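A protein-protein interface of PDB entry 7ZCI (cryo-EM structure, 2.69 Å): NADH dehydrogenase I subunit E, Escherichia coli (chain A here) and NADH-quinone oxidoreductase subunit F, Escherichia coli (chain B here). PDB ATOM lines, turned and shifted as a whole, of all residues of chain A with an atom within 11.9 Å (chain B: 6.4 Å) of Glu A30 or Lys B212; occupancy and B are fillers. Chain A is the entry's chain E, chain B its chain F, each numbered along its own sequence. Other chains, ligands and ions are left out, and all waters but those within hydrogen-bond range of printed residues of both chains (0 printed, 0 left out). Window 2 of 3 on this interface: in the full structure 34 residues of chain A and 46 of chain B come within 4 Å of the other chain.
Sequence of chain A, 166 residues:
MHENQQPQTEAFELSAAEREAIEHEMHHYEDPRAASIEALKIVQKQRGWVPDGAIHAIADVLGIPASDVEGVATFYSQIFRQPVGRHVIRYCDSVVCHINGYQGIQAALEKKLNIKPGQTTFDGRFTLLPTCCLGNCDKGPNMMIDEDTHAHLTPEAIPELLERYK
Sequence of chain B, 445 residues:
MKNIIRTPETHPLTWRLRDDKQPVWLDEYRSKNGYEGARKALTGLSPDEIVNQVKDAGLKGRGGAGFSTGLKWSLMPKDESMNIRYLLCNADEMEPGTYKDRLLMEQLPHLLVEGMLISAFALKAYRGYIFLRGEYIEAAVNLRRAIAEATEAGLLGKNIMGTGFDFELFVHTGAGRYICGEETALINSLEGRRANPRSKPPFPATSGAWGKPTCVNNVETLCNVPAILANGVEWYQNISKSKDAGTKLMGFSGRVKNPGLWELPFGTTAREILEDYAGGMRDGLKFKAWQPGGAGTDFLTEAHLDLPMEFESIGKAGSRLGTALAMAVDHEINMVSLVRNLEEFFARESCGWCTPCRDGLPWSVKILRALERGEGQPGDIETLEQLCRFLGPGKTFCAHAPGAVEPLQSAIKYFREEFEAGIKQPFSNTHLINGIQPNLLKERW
O of His A28 touches CZ of Arg B127, at 3.9 Å.
Tyr B129 touches Tyr A29 (CE1 to CE1, 3.6 Å).
OE2 of Glu A30 touches CB of Trp B210 (3.3 Å).
Asp A31 touches Trp B210 (CB to NE1, 3.5 Å).
CB of Ala A34 touches CZ2 of Trp B210 (3.8 Å).
OH of Tyr B126 is in hydrogen-bond range of NH1 of Arg B127 (3.1 Å).
The side-chain hydroxyl (OH) of Tyr B86 sits at hydrogen-bond distance from the side-chain hydroxyl (OH) of Tyr B126 (3.3 Å).
O of Trp B210 is in hydrogen-bond range of NZ of Lys B212, at 2.9 Å.
O of Arg B85 is in hydrogen-bond range of N of Arg B127 (3.2 Å).
OD1 of Asp A31 sits at hydrogen-bond distance from N of Arg A33.
The backbone NH of Tyr B86 sits at hydrogen-bond distance from the backbone carbonyl oxygen of Pro B213.
The side-chain carboxylate of Glu A30 lies within salt-bridge range of the side-chain amino group of Lys B212 (2.9 Å).
OH of Tyr B86 sits at hydrogen-bond distance from OE1 of Glu A30 (2.6 Å).
The backbone carbonyl oxygen of His A28 is in hydrogen-bond range of the side-chain hydroxyl of Tyr B129.
Hydrophobic or aromatic side chains of chain A that line the printed part of chain B: Tyr A29 and Ala A34.
Hydrophobic or aromatic side chains of chain B within 4 Å of the printed part of chain A: Tyr B86, Tyr B129 and Trp B210.
Among the printed residues, Asp or Glu carboxylates within 4 Å of a Lys or Arg side-chain nitrogen of the other chain: Glu A30 with Lys B212 (2.9 Å).
Of the printed residues of chain B, Asp A31 touches Trp B210.
Leu A62 touches none of the printed residues of chain B.
Ile A64 touches none of the printed residues of chain B.
No residue of chain A comes within 4 Å of Ile B84.
Of the printed residues of chain A, Arg B127 touches His A28 (3.9 Å).
No residue of chain A comes within 4 Å of Ala B205.
No residue of chain A comes within 4 Å of Ser B207.
No residue of chain A comes within 4 Å of Gly B208.
Printed residues of chain A within 4 Å of Trp B210: Glu A30 (3.3 Å), Asp A31 (3.5 Å) and Ala A34 (3.8 Å).
Gly B211 touches none of the printed residues of chain A.
No residue of chain A comes within 4 Å of Pro B213.
No residue of chain A comes within 4 Å of Thr B214.
The nearest residue of chain B that does not touch Glu A30 is Ile B84 (4.1 Å).
The nearest printed residue of chain A that does not touch Arg B127 is His A27 (4.02 Å).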
ATOM      1  N   ILE A  22       5.293  -7.747 -12.410  1.00  0.00           N
ATOM      2  CA  ILE A  22       4.412  -8.905 -12.313  1.00  0.00           C
ATOM      3  C   ILE A  22       2.993  -8.541 -12.734  1.00  0.00           C
ATOM      4  O   ILE A  22       2.345  -9.289 -13.474  1.00  0.00           O
ATOM      5  CB  ILE A  22       4.461  -9.493 -10.892  1.00  0.00           C
ATOM      6  CG1 ILE A  22       5.791 -10.202 -10.662  1.00  0.00           C
ATOM      7  CG2 ILE A  22       3.347 -10.482 -10.681  1.00  0.00           C
ATOM      8  CD1 ILE A  22       6.119 -10.435  -9.211  1.00  0.00           C
ATOM      9  N   GLU A  23       2.496  -7.378 -12.305  1.00  0.00           N
ATOM     10  CA  GLU A  23       1.144  -6.976 -12.682  1.00  0.00           C
ATOM     11  C   GLU A  23       1.044  -6.673 -14.175  1.00  0.00           C
ATOM     12  O   GLU A  23       0.033  -7.001 -14.818  1.00  0.00           O
ATOM     13  CB  GLU A  23       0.714  -5.776 -11.847  1.00  0.00           C
ATOM     14  CG  GLU A  23       0.494  -6.120 -10.386  1.00  0.00           C
ATOM     15  CD  GLU A  23       0.537  -4.904  -9.487  1.00  0.00           C
ATOM     16  OE1 GLU A  23       0.906  -3.817  -9.979  1.00  0.00           O
ATOM     17  OE2 GLU A  23       0.214  -5.034  -8.288  1.00  0.00           O
ATOM     18  N   HIS A  24       2.089  -6.069 -14.747  1.00  0.00           N
ATOM     19  CA  HIS A  24       2.111  -5.833 -16.185  1.00  0.00           C
ATOM     20  C   HIS A  24       2.112  -7.144 -16.957  1.00  0.00           C
ATOM     21  O   HIS A  24       1.498  -7.242 -18.024  1.00  0.00           O
ATOM     22  CB  HIS A  24       3.327  -4.992 -16.560  1.00  0.00           C
ATOM     23  CG  HIS A  24       3.435  -4.712 -18.025  1.00  0.00           C
ATOM     24  ND1 HIS A  24       2.442  -4.072 -18.734  1.00  0.00           N
ATOM     25  CD2 HIS A  24       4.413  -4.993 -18.917  1.00  0.00           C
ATOM     26  CE1 HIS A  24       2.806  -3.967 -20.000  1.00  0.00           C
ATOM     27  NE2 HIS A  24       3.997  -4.519 -20.137  1.00  0.00           N
ATOM     28  N   GLU A  25       2.797  -8.162 -16.436  1.00  0.00           N
ATOM     29  CA  GLU A  25       2.715  -9.480 -17.055  1.00  0.00           C
ATOM     30  C   GLU A  25       1.337 -10.101 -16.875  1.00  0.00           C
ATOM     31  O   GLU A  25       0.880 -10.847 -17.745  1.00  0.00           O
ATOM     32  CB  GLU A  25       3.783 -10.402 -16.479  1.00  0.00           C
ATOM     33  CG  GLU A  25       5.149 -10.182 -17.086  1.00  0.00           C
ATOM     34  CD  GLU A  25       5.210 -10.564 -18.550  1.00  0.00           C
ATOM     35  OE1 GLU A  25       4.580 -11.570 -18.938  1.00  0.00           O
ATOM     36  OE2 GLU A  25       5.901  -9.860 -19.315  1.00  0.00           O
ATOM     37  N   MET A  26       0.672  -9.819 -15.752  1.00  0.00           N
ATOM     38  CA  MET A  26      -0.677 -10.331 -15.534  1.00  0.00           C
ATOM     39  C   MET A  26      -1.679  -9.724 -16.502  1.00  0.00           C
ATOM     40  O   MET A  26      -2.688 -10.363 -16.819  1.00  0.00           O
ATOM     41  CB  MET A  26      -1.128 -10.080 -14.096  1.00  0.00           C
ATOM     42  CG  MET A  26      -0.410 -10.909 -13.060  1.00  0.00           C
ATOM     43  SD  MET A  26      -0.653 -10.300 -11.385  1.00  0.00           S
ATOM     44  CE  MET A  26      -2.368  -9.813 -11.447  1.00  0.00           C
ATOM     45  N   HIS A  27      -1.432  -8.500 -16.978  1.00  0.00           N
ATOM     46  CA  HIS A  27      -2.322  -7.911 -17.979  1.00  0.00           C
ATOM     47  C   HIS A  27      -2.301  -8.655 -19.309  1.00  0.00           C
ATOM     48  O   HIS A  27      -3.255  -8.536 -20.081  1.00  0.00           O
ATOM     49  CB  HIS A  27      -1.965  -6.446 -18.231  1.00  0.00           C
ATOM     50  CG  HIS A  27      -2.087  -5.576 -17.022  1.00  0.00           C
ATOM     51  ND1 HIS A  27      -1.434  -4.368 -16.908  1.00  0.00           N
ATOM     52  CD2 HIS A  27      -2.780  -5.740 -15.871  1.00  0.00           C
ATOM     53  CE1 HIS A  27      -1.720  -3.824 -15.738  1.00  0.00           C
ATOM     54  NE2 HIS A  27      -2.535  -4.637 -15.090  1.00  0.00           N
ATOM     55  N   HIS A  28      -1.247  -9.415 -19.595  1.00  0.00           N
ATOM     56  CA  HIS A  28      -1.087 -10.057 -20.893  1.00  0.00           C
ATOM     57  C   HIS A  28      -1.937 -11.306 -21.062  1.00  0.00           C
ATOM     58  O   HIS A  28      -1.996 -11.846 -22.170  1.00  0.00           O
ATOM     59  CB  HIS A  28       0.379 -10.427 -21.112  1.00  0.00           C
ATOM     60  CG  HIS A  28       1.303  -9.252 -21.128  1.00  0.00           C
ATOM     61  ND1 HIS A  28       2.659  -9.370 -20.919  1.00  0.00           N
ATOM     62  CD2 HIS A  28       1.069  -7.935 -21.336  1.00  0.00           C
ATOM     63  CE1 HIS A  28       3.219  -8.177 -20.990  1.00  0.00           C
ATOM     64  NE2 HIS A  28       2.276  -7.289 -21.242  1.00  0.00           N
ATOM     65  N   TYR A  29      -2.584 -11.785 -20.006  1.00  0.00           N
ATOM     66  CA  TYR A  29      -3.214 -13.093 -20.027  1.00  0.00           C
ATOM     67  C   TYR A  29      -4.652 -13.007 -19.545  1.00  0.00           C
ATOM     68  O   TYR A  29      -5.013 -12.134 -18.754  1.00  0.00           O
ATOM     69  CB  TYR A  29      -2.443 -14.088 -19.159  1.00  0.00           C
ATOM     70  CG  TYR A  29      -1.010 -14.274 -19.581  1.00  0.00           C
ATOM     71  CD1 TYR A  29      -0.687 -15.036 -20.692  1.00  0.00           C
ATOM     72  CD2 TYR A  29       0.019 -13.688 -18.869  1.00  0.00           C
ATOM     73  CE1 TYR A  29       0.619 -15.201 -21.081  1.00  0.00           C
ATOM     74  CE2 TYR A  29       1.327 -13.851 -19.249  1.00  0.00           C
ATOM     75  CZ  TYR A  29       1.622 -14.608 -20.356  1.00  0.00           C
ATOM     76  OH  TYR A  29       2.930 -14.767 -20.736  1.00  0.00           O
ATOM     77  N   GLU A  30      -5.464 -13.936 -20.044  1.00  0.00           N
ATOM     78  CA  GLU A  30      -6.852 -14.047 -19.615  1.00  0.00           C
ATOM     79  C   GLU A  30      -6.952 -14.438 -18.144  1.00  0.00           C
ATOM     80  O   GLU A  30      -7.791 -13.907 -17.408  1.00  0.00           O
ATOM     81  CB  GLU A  30      -7.564 -15.061 -20.507  1.00  0.00           C
ATOM     82  CG  GLU A  30      -8.726 -15.783 -19.887  1.00  0.00           C
ATOM     83  CD  GLU A  30      -9.317 -16.794 -20.836  1.00  0.00           C
ATOM     84  OE1 GLU A  30      -9.070 -16.668 -22.051  1.00  0.00           O
ATOM     85  OE2 GLU A  30     -10.029 -17.704 -20.371  1.00  0.00           O
ATOM     86  N   ASP A  31      -6.102 -15.356 -17.699  1.00  0.00           N
ATOM     87  CA  ASP A  31      -6.069 -15.814 -16.324  1.00  0.00           C
ATOM     88  C   ASP A  31      -4.788 -15.314 -15.679  1.00  0.00           C
ATOM     89  O   ASP A  31      -3.722 -15.404 -16.300  1.00  0.00           O
ATOM     90  CB  ASP A  31      -6.135 -17.351 -16.281  1.00  0.00           C
ATOM     91  CG  ASP A  31      -6.382 -17.916 -14.887  1.00  0.00           C
ATOM     92  OD1 ASP A  31      -5.681 -17.565 -13.924  1.00  0.00           O
ATOM     93  OD2 ASP A  31      -7.296 -18.752 -14.760  1.00  0.00           O
ATOM     94  N   PRO A  32      -4.845 -14.759 -14.464  1.00  0.00           N
ATOM     95  CA  PRO A  32      -3.611 -14.298 -13.806  1.00  0.00           C
ATOM     96  C   PRO A  32      -2.638 -15.409 -13.442  1.00  0.00           C
ATOM     97  O   PRO A  32      -1.468 -15.104 -13.194  1.00  0.00           O
ATOM     98  CB  PRO A  32      -4.128 -13.582 -12.552  1.00  0.00           C
ATOM     99  CG  PRO A  32      -5.494 -14.116 -12.343  1.00  0.00           C
ATOM    100  CD  PRO A  32      -6.041 -14.373 -13.705  1.00  0.00           C
ATOM    101  N   ARG A  33      -3.078 -16.674 -13.399  1.00  0.00           N
ATOM    102  CA  ARG A  33      -2.176 -17.790 -13.110  1.00  0.00           C
ATOM    103  C   ARG A  33      -1.089 -17.921 -14.167  1.00  0.00           C
ATOM    104  O   ARG A  33       0.026 -18.355 -13.864  1.00  0.00           O
ATOM    105  CB  ARG A  33      -2.980 -19.090 -13.010  1.00  0.00           C
ATOM    106  CG  ARG A  33      -2.179 -20.353 -12.739  1.00  0.00           C
ATOM    107  CD  ARG A  33      -3.021 -21.600 -12.944  1.00  0.00           C
ATOM    108  NE  ARG A  33      -4.081 -21.678 -11.951  1.00  0.00           N
ATOM    109  CZ  ARG A  33      -3.940 -22.207 -10.744  1.00  0.00           C
ATOM    110  NH1 ARG A  33      -2.809 -22.779 -10.370  1.00  0.00           N
ATOM    111  NH2 ARG A  33      -4.957 -22.155  -9.893  1.00  0.00           N
ATOM    112  N   ALA A  34      -1.373 -17.484 -15.391  1.00  0.00           N
ATOM    113  CA  ALA A  34      -0.454 -17.601 -16.512  1.00  0.00           C
ATOM    114  C   ALA A  34       0.775 -16.710 -16.388  1.00  0.00           C
ATOM    115  O   ALA A  34       1.681 -16.826 -17.218  1.00  0.00           O
ATOM    116  CB  ALA A  34      -1.189 -17.292 -17.808  1.00  0.00           C
ATOM    117  N   ALA A  35       0.834 -15.831 -15.393  1.00  0.00           N
ATOM    118  CA  ALA A  35       2.008 -15.008 -15.152  1.00  0.00           C
ATOM    119  C   ALA A  35       2.926 -15.582 -14.080  1.00  0.00           C
ATOM    120  O   ALA A  35       3.829 -14.880 -13.628  1.00  0.00           O
ATOM    121  CB  ALA A  35       1.591 -13.591 -14.767  1.00  0.00           C
ATOM    122  N   SER A  36       2.732 -16.838 -13.675  1.00  0.00           N
ATOM    123  CA  SER A  36       3.525 -17.397 -12.582  1.00  0.00           C
ATOM    124  C   SER A  36       4.977 -17.611 -12.986  1.00  0.00           C
ATOM    125  O   SER A  36       5.891 -17.279 -12.221  1.00  0.00           O
ATOM    126  CB  SER A  36       2.908 -18.708 -12.105  1.00  0.00           C
ATOM    127  OG  SER A  36       2.974 -19.688 -13.117  1.00  0.00           O
ATOM    128  N   LEU A  62      -0.553 -13.090  -7.349  1.00  0.00           N
ATOM    129  CA  LEU A  62      -1.266 -13.723  -8.448  1.00  0.00           C
ATOM    130  C   LEU A  62      -2.630 -14.278  -8.061  1.00  0.00           C
ATOM    131  O   LEU A  62      -3.462 -14.494  -8.945  1.00  0.00           O
ATOM    132  CB  LEU A  62      -0.425 -14.849  -9.034  1.00  0.00           C
ATOM    133  CG  LEU A  62       0.316 -14.525 -10.323  1.00  0.00           C
ATOM    134  CD1 LEU A  62       1.494 -13.630 -10.059  1.00  0.00           C
ATOM    135  CD2 LEU A  62       0.763 -15.810 -10.926  1.00  0.00           C
ATOM    136  N   GLY A  63      -2.882 -14.518  -6.780  1.00  0.00           N
ATOM    137  CA  GLY A  63      -4.147 -15.101  -6.388  1.00  0.00           C
ATOM    138  C   GLY A  63      -4.248 -16.595  -6.572  1.00  0.00           C
ATOM    139  O   GLY A  63      -5.359 -17.121  -6.667  1.00  0.00           O
ATOM    140  N   ILE A  64      -3.126 -17.295  -6.640  1.00  0.00           N
ATOM    141  CA  ILE A  64      -3.100 -18.750  -6.745  1.00  0.00           C
ATOM    142  C   ILE A  64      -2.453 -19.277  -5.472  1.00  0.00           C
ATOM    143  O   ILE A  64      -1.799 -18.513  -4.745  1.00  0.00           O
ATOM    144  CB  ILE A  64      -2.367 -19.220  -8.024  1.00  0.00           C
ATOM    145  CG1 ILE A  64      -0.921 -18.733  -8.040  1.00  0.00           C
ATOM    146  CG2 ILE A  64      -3.107 -18.747  -9.260  1.00  0.00           C
ATOM    147  CD1 ILE A  64      -0.148 -19.227  -9.240  1.00  0.00           C
ATOM    148  N   ILE B  84     -12.760 -16.269 -28.780  1.00  0.00           N
ATOM    149  CA  ILE B  84     -11.660 -15.984 -27.864  1.00  0.00           C
ATOM    150  C   ILE B  84     -10.490 -16.848 -28.324  1.00  0.00           C
ATOM    151  O   ILE B  84      -9.759 -17.433 -27.518  1.00  0.00           O
ATOM    152  CB  ILE B  84     -12.057 -16.234 -26.394  1.00  0.00           C
ATOM    153  CG1 ILE B  84     -13.402 -15.587 -26.084  1.00  0.00           C
ATOM    154  CG2 ILE B  84     -11.089 -15.562 -25.431  1.00  0.00           C
ATOM    155  CD1 ILE B  84     -13.438 -14.090 -26.319  1.00  0.00           C
ATOM    156  N   ARG B  85     -10.342 -16.985 -29.634  1.00  0.00           N
ATOM    157  CA  ARG B  85      -9.410 -17.951 -30.192  1.00  0.00           C
ATOM    158  C   ARG B  85      -7.952 -17.497 -30.096  1.00  0.00           C
ATOM    159  O   ARG B  85      -7.614 -16.296 -30.156  1.00  0.00           O
ATOM    160  CB  ARG B  85      -9.785 -18.253 -31.637  1.00  0.00           C
ATOM    161  CG  ARG B  85     -11.244 -18.590 -31.778  1.00  0.00           C
ATOM    162  CD  ARG B  85     -11.583 -19.153 -33.126  1.00  0.00           C
ATOM    163  NE  ARG B  85     -12.927 -19.708 -33.115  1.00  0.00           N
ATOM    164  CZ  ARG B  85     -13.461 -20.404 -34.105  1.00  0.00           C
ATOM    165  NH1 ARG B  85     -12.784 -20.664 -35.211  1.00  0.00           N
ATOM    166  NH2 ARG B  85     -14.705 -20.857 -33.982  1.00  0.00           N
ATOM    167  N   TYR B  86      -7.084 -18.497 -29.942  1.00  0.00           N
ATOM    168  CA  TYR B  86      -5.664 -18.292 -29.710  1.00  0.00           C
ATOM    169  C   TYR B  86      -4.832 -18.999 -30.771  1.00  0.00           C
ATOM    170  O   TYR B  86      -5.122 -20.136 -31.160  1.00  0.00           O
ATOM    171  CB  TYR B  86      -5.263 -18.792 -28.333  1.00  0.00           C
ATOM    172  CG  TYR B  86      -5.889 -18.023 -27.201  1.00  0.00           C
ATOM    173  CD1 TYR B  86      -5.469 -16.739 -26.898  1.00  0.00           C
ATOM    174  CD2 TYR B  86      -6.892 -18.585 -26.430  1.00  0.00           C
ATOM    175  CE1 TYR B  86      -6.036 -16.036 -25.864  1.00  0.00           C
ATOM    176  CE2 TYR B  86      -7.461 -17.887 -25.391  1.00  0.00           C
ATOM    177  CZ  TYR B  86      -7.033 -16.613 -25.117  1.00  0.00           C
ATOM    178  OH  TYR B  86      -7.593 -15.909 -24.084  1.00  0.00           O
ATOM    179  N   TYR B 126      -8.138 -14.020 -31.959  1.00  0.00           N
ATOM    180  CA  TYR B 126      -7.963 -12.671 -31.460  1.00  0.00           C
ATOM    181  C   TYR B 126      -6.624 -12.490 -30.772  1.00  0.00           C
ATOM    182  O   TYR B 126      -6.134 -11.360 -30.707  1.00  0.00           O
ATOM    183  CB  TYR B 126      -9.113 -12.310 -30.520  1.00  0.00           C
ATOM    184  CG  TYR B 126      -8.815 -12.435 -29.046  1.00  0.00           C
ATOM    185  CD1 TYR B 126      -8.728 -13.679 -28.439  1.00  0.00           C
ATOM    186  CD2 TYR B 126      -8.657 -11.309 -28.255  1.00  0.00           C
ATOM    187  CE1 TYR B 126      -8.466 -13.795 -27.096  1.00  0.00           C
ATOM    188  CE2 TYR B 126      -8.401 -11.419 -26.910  1.00  0.00           C
ATOM    189  CZ  TYR B 126      -8.308 -12.664 -26.337  1.00  0.00           C
ATOM    190  OH  TYR B 126      -8.050 -12.783 -24.994  1.00  0.00           O
ATOM    191  N   ARG B 127      -6.005 -13.559 -30.266  1.00  0.00           N
ATOM    192  CA  ARG B 127      -4.712 -13.360 -29.622  1.00  0.00           C
ATOM    193  C   ARG B 127      -3.691 -14.372 -30.114  1.00  0.00           C
ATOM    194  O   ARG B 127      -4.036 -15.467 -30.566  1.00  0.00           O
ATOM    195  CB  ARG B 127      -4.822 -13.421 -28.102  1.00  0.00           C
ATOM    196  CG  ARG B 127      -4.501 -12.106 -27.428  1.00  0.00           C
ATOM    197  CD  ARG B 127      -4.895 -12.124 -25.974  1.00  0.00           C
ATOM    198  NE  ARG B 127      -4.711 -10.823 -25.349  1.00  0.00           N
ATOM    199  CZ  ARG B 127      -5.147 -10.505 -24.138  1.00  0.00           C
ATOM    200  NH1 ARG B 127      -5.806 -11.374 -23.392  1.00  0.00           N
ATOM    201  NH2 ARG B 127      -4.911  -9.287 -23.662  1.00  0.00           N
ATOM    202  N   TYR B 129       0.375 -15.937 -29.147  1.00  0.00           N
ATOM    203  CA  TYR B 129       1.522 -16.023 -28.259  1.00  0.00           C
ATOM    204  C   TYR B 129       2.649 -16.768 -28.951  1.00  0.00           C
ATOM    205  O   TYR B 129       2.416 -17.791 -29.592  1.00  0.00           O
ATOM    206  CB  TYR B 129       1.168 -16.735 -26.959  1.00  0.00           C
ATOM    207  CG  TYR B 129       0.140 -16.027 -26.124  1.00  0.00           C
ATOM    208  CD1 TYR B 129       0.518 -15.079 -25.194  1.00  0.00           C
ATOM    209  CD2 TYR B 129      -1.208 -16.317 -26.253  1.00  0.00           C
ATOM    210  CE1 TYR B 129      -0.409 -14.438 -24.426  1.00  0.00           C
ATOM    211  CE2 TYR B 129      -2.145 -15.676 -25.487  1.00  0.00           C
ATOM    212  CZ  TYR B 129      -1.737 -14.736 -24.576  1.00  0.00           C
ATOM    213  OH  TYR B 129      -2.659 -14.087 -23.798  1.00  0.00           O
ATOM    214  N   PRO B 204      -6.627 -29.510 -29.054  1.00  0.00           N
ATOM    215  CA  PRO B 204      -6.626 -28.083 -28.702  1.00  0.00           C
ATOM    216  C   PRO B 204      -7.415 -27.202 -29.651  1.00  0.00           C
ATOM    217  O   PRO B 204      -7.768 -26.083 -29.265  1.00  0.00           O
ATOM    218  CB  PRO B 204      -5.137 -27.725 -28.719  1.00  0.00           C
ATOM    219  CG  PRO B 204      -4.458 -28.987 -28.422  1.00  0.00           C
ATOM    220  CD  PRO B 204      -5.256 -30.046 -29.103  1.00  0.00           C
ATOM    221  N   ALA B 205      -7.703 -27.668 -30.869  1.00  0.00           N
ATOM    222  CA  ALA B 205      -8.515 -26.891 -31.801  1.00  0.00           C
ATOM    223  C   ALA B 205      -9.914 -26.639 -31.263  1.00  0.00           C
ATOM    224  O   ALA B 205     -10.514 -25.605 -31.570  1.00  0.00           O
ATOM    225  CB  ALA B 205      -8.593 -27.597 -33.152  1.00  0.00           C
ATOM    226  N   THR B 206     -10.452 -27.555 -30.463  1.00  0.00           N
ATOM    227  CA  THR B 206     -11.759 -27.362 -29.851  1.00  0.00           C
ATOM    228  C   THR B 206     -11.679 -26.873 -28.414  1.00  0.00           C
ATOM    229  O   THR B 206     -12.494 -26.045 -28.000  1.00  0.00           O
ATOM    230  CB  THR B 206     -12.569 -28.659 -29.900  1.00  0.00           C
ATOM    231  OG1 THR B 206     -11.895 -29.679 -29.155  1.00  0.00           O
ATOM    232  CG2 THR B 206     -12.741 -29.116 -31.330  1.00  0.00           C
ATOM    233  N   SER B 207     -10.717 -27.366 -27.639  1.00  0.00           N
ATOM    234  CA  SER B 207     -10.559 -26.987 -26.234  1.00  0.00           C
ATOM    235  C   SER B 207      -9.062 -26.917 -25.950  1.00  0.00           C
ATOM    236  O   SER B 207      -8.435 -27.925 -25.620  1.00  0.00           O
ATOM    237  CB  SER B 207     -11.262 -27.974 -25.316  1.00  0.00           C
ATOM    238  OG  SER B 207     -11.055 -27.630 -23.961  1.00  0.00           O
ATOM    239  N   GLY B 208      -8.497 -25.724 -26.074  1.00  0.00           N
ATOM    240  CA  GLY B 208      -7.072 -25.567 -25.901  1.00  0.00           C
ATOM    241  C   GLY B 208      -6.695 -24.656 -24.759  1.00  0.00           C
ATOM    242  O   GLY B 208      -6.951 -24.975 -23.597  1.00  0.00           O
ATOM    243  N   ALA B 209      -6.077 -23.524 -25.081  1.00  0.00           N
ATOM    244  CA  ALA B 209      -5.613 -22.593 -24.064  1.00  0.00           C
ATOM    245  C   ALA B 209      -6.802 -21.951 -23.372  1.00  0.00           C
ATOM    246  O   ALA B 209      -7.624 -21.295 -24.019  1.00  0.00           O
ATOM    247  CB  ALA B 209      -4.706 -21.540 -24.689  1.00  0.00           C
ATOM    248  N   TRP B 210      -6.896 -22.173 -22.059  1.00  0.00           N
ATOM    249  CA  TRP B 210      -7.997 -21.705 -21.214  1.00  0.00           C
ATOM    250  C   TRP B 210      -9.351 -22.207 -21.708  1.00  0.00           C
ATOM    251  O   TRP B 210     -10.371 -21.542 -21.541  1.00  0.00           O
ATOM    252  CB  TRP B 210      -7.998 -20.181 -21.087  1.00  0.00           C
ATOM    253  CG  TRP B 210      -6.718 -19.636 -20.541  1.00  0.00           C
ATOM    254  CD1 TRP B 210      -6.318 -19.640 -19.244  1.00  0.00           C
ATOM    255  CD2 TRP B 210      -5.668 -19.013 -21.283  1.00  0.00           C
ATOM    256  NE1 TRP B 210      -5.085 -19.060 -19.127  1.00  0.00           N
ATOM    257  CE2 TRP B 210      -4.664 -18.662 -20.366  1.00  0.00           C
ATOM    258  CE3 TRP B 210      -5.483 -18.712 -22.631  1.00  0.00           C
ATOM    259  CZ2 TRP B 210      -3.490 -18.026 -20.756  1.00  0.00           C
ATOM    260  CZ3 TRP B 210      -4.319 -18.082 -23.017  1.00  0.00           C
ATOM    261  CH2 TRP B 210      -3.338 -17.745 -22.083  1.00  0.00           C
ATOM    262  N   GLY B 211      -9.369 -23.389 -22.316  1.00  0.00           N
ATOM    263  CA  GLY B 211     -10.593 -23.985 -22.799  1.00  0.00           C
ATOM    264  C   GLY B 211     -11.101 -23.445 -24.114  1.00  0.00           C
ATOM    265  O   GLY B 211     -12.146 -23.907 -24.586  1.00  0.00           O
ATOM    266  N   LYS B 212     -10.416 -22.495 -24.710  1.00  0.00           N
ATOM    267  CA  LYS B 212     -10.814 -21.867 -25.958  1.00  0.00           C
ATOM    268  C   LYS B 212     -10.223 -22.611 -27.143  1.00  0.00           C
ATOM    269  O   LYS B 212      -9.299 -23.411 -26.986  1.00  0.00           O
ATOM    270  CB  LYS B 212     -10.359 -20.412 -25.981  1.00  0.00           C
ATOM    271  CG  LYS B 212     -10.727 -19.619 -24.750  1.00  0.00           C
ATOM    272  CD  LYS B 212     -12.221 -19.627 -24.527  1.00  0.00           C
ATOM    273  CE  LYS B 212     -12.589 -18.776 -23.332  1.00  0.00           C
ATOM    274  NZ  LYS B 212     -11.766 -19.109 -22.144  1.00  0.00           N
ATOM    275  N   PRO B 213     -10.778 -22.414 -28.336  1.00  0.00           N
ATOM    276  CA  PRO B 213     -10.108 -22.899 -29.547  1.00  0.00           C
ATOM    277  C   PRO B 213      -8.705 -22.322 -29.683  1.00  0.00           C
ATOM    278  O   PRO B 213      -8.493 -21.105 -29.636  1.00  0.00           O
ATOM    279  CB  PRO B 213     -11.035 -22.434 -30.677  1.00  0.00           C
ATOM    280  CG  PRO B 213     -12.177 -21.724 -30.022  1.00  0.00           C
ATOM    281  CD  PRO B 213     -12.189 -22.102 -28.593  1.00  0.00           C
ATOM    282  N   THR B 214      -7.743 -23.222 -29.843  1.00  0.00           N
ATOM    283  CA  THR B 214      -6.330 -22.895 -29.854  1.00  0.00           C
ATOM    284  C   THR B 214      -5.661 -23.678 -30.967  1.00  0.00           C
ATOM    285  O   THR B 214      -5.957 -24.857 -31.167  1.00  0.00           O
ATOM    286  CB  THR B 214      -5.669 -23.238 -28.518  1.00  0.00           C
ATOM    287  OG1 THR B 214      -6.471 -22.739 -27.445  1.00  0.00           O
ATOM    288  CG2 THR B 214      -4.311 -22.617 -28.429  1.00  0.00           C
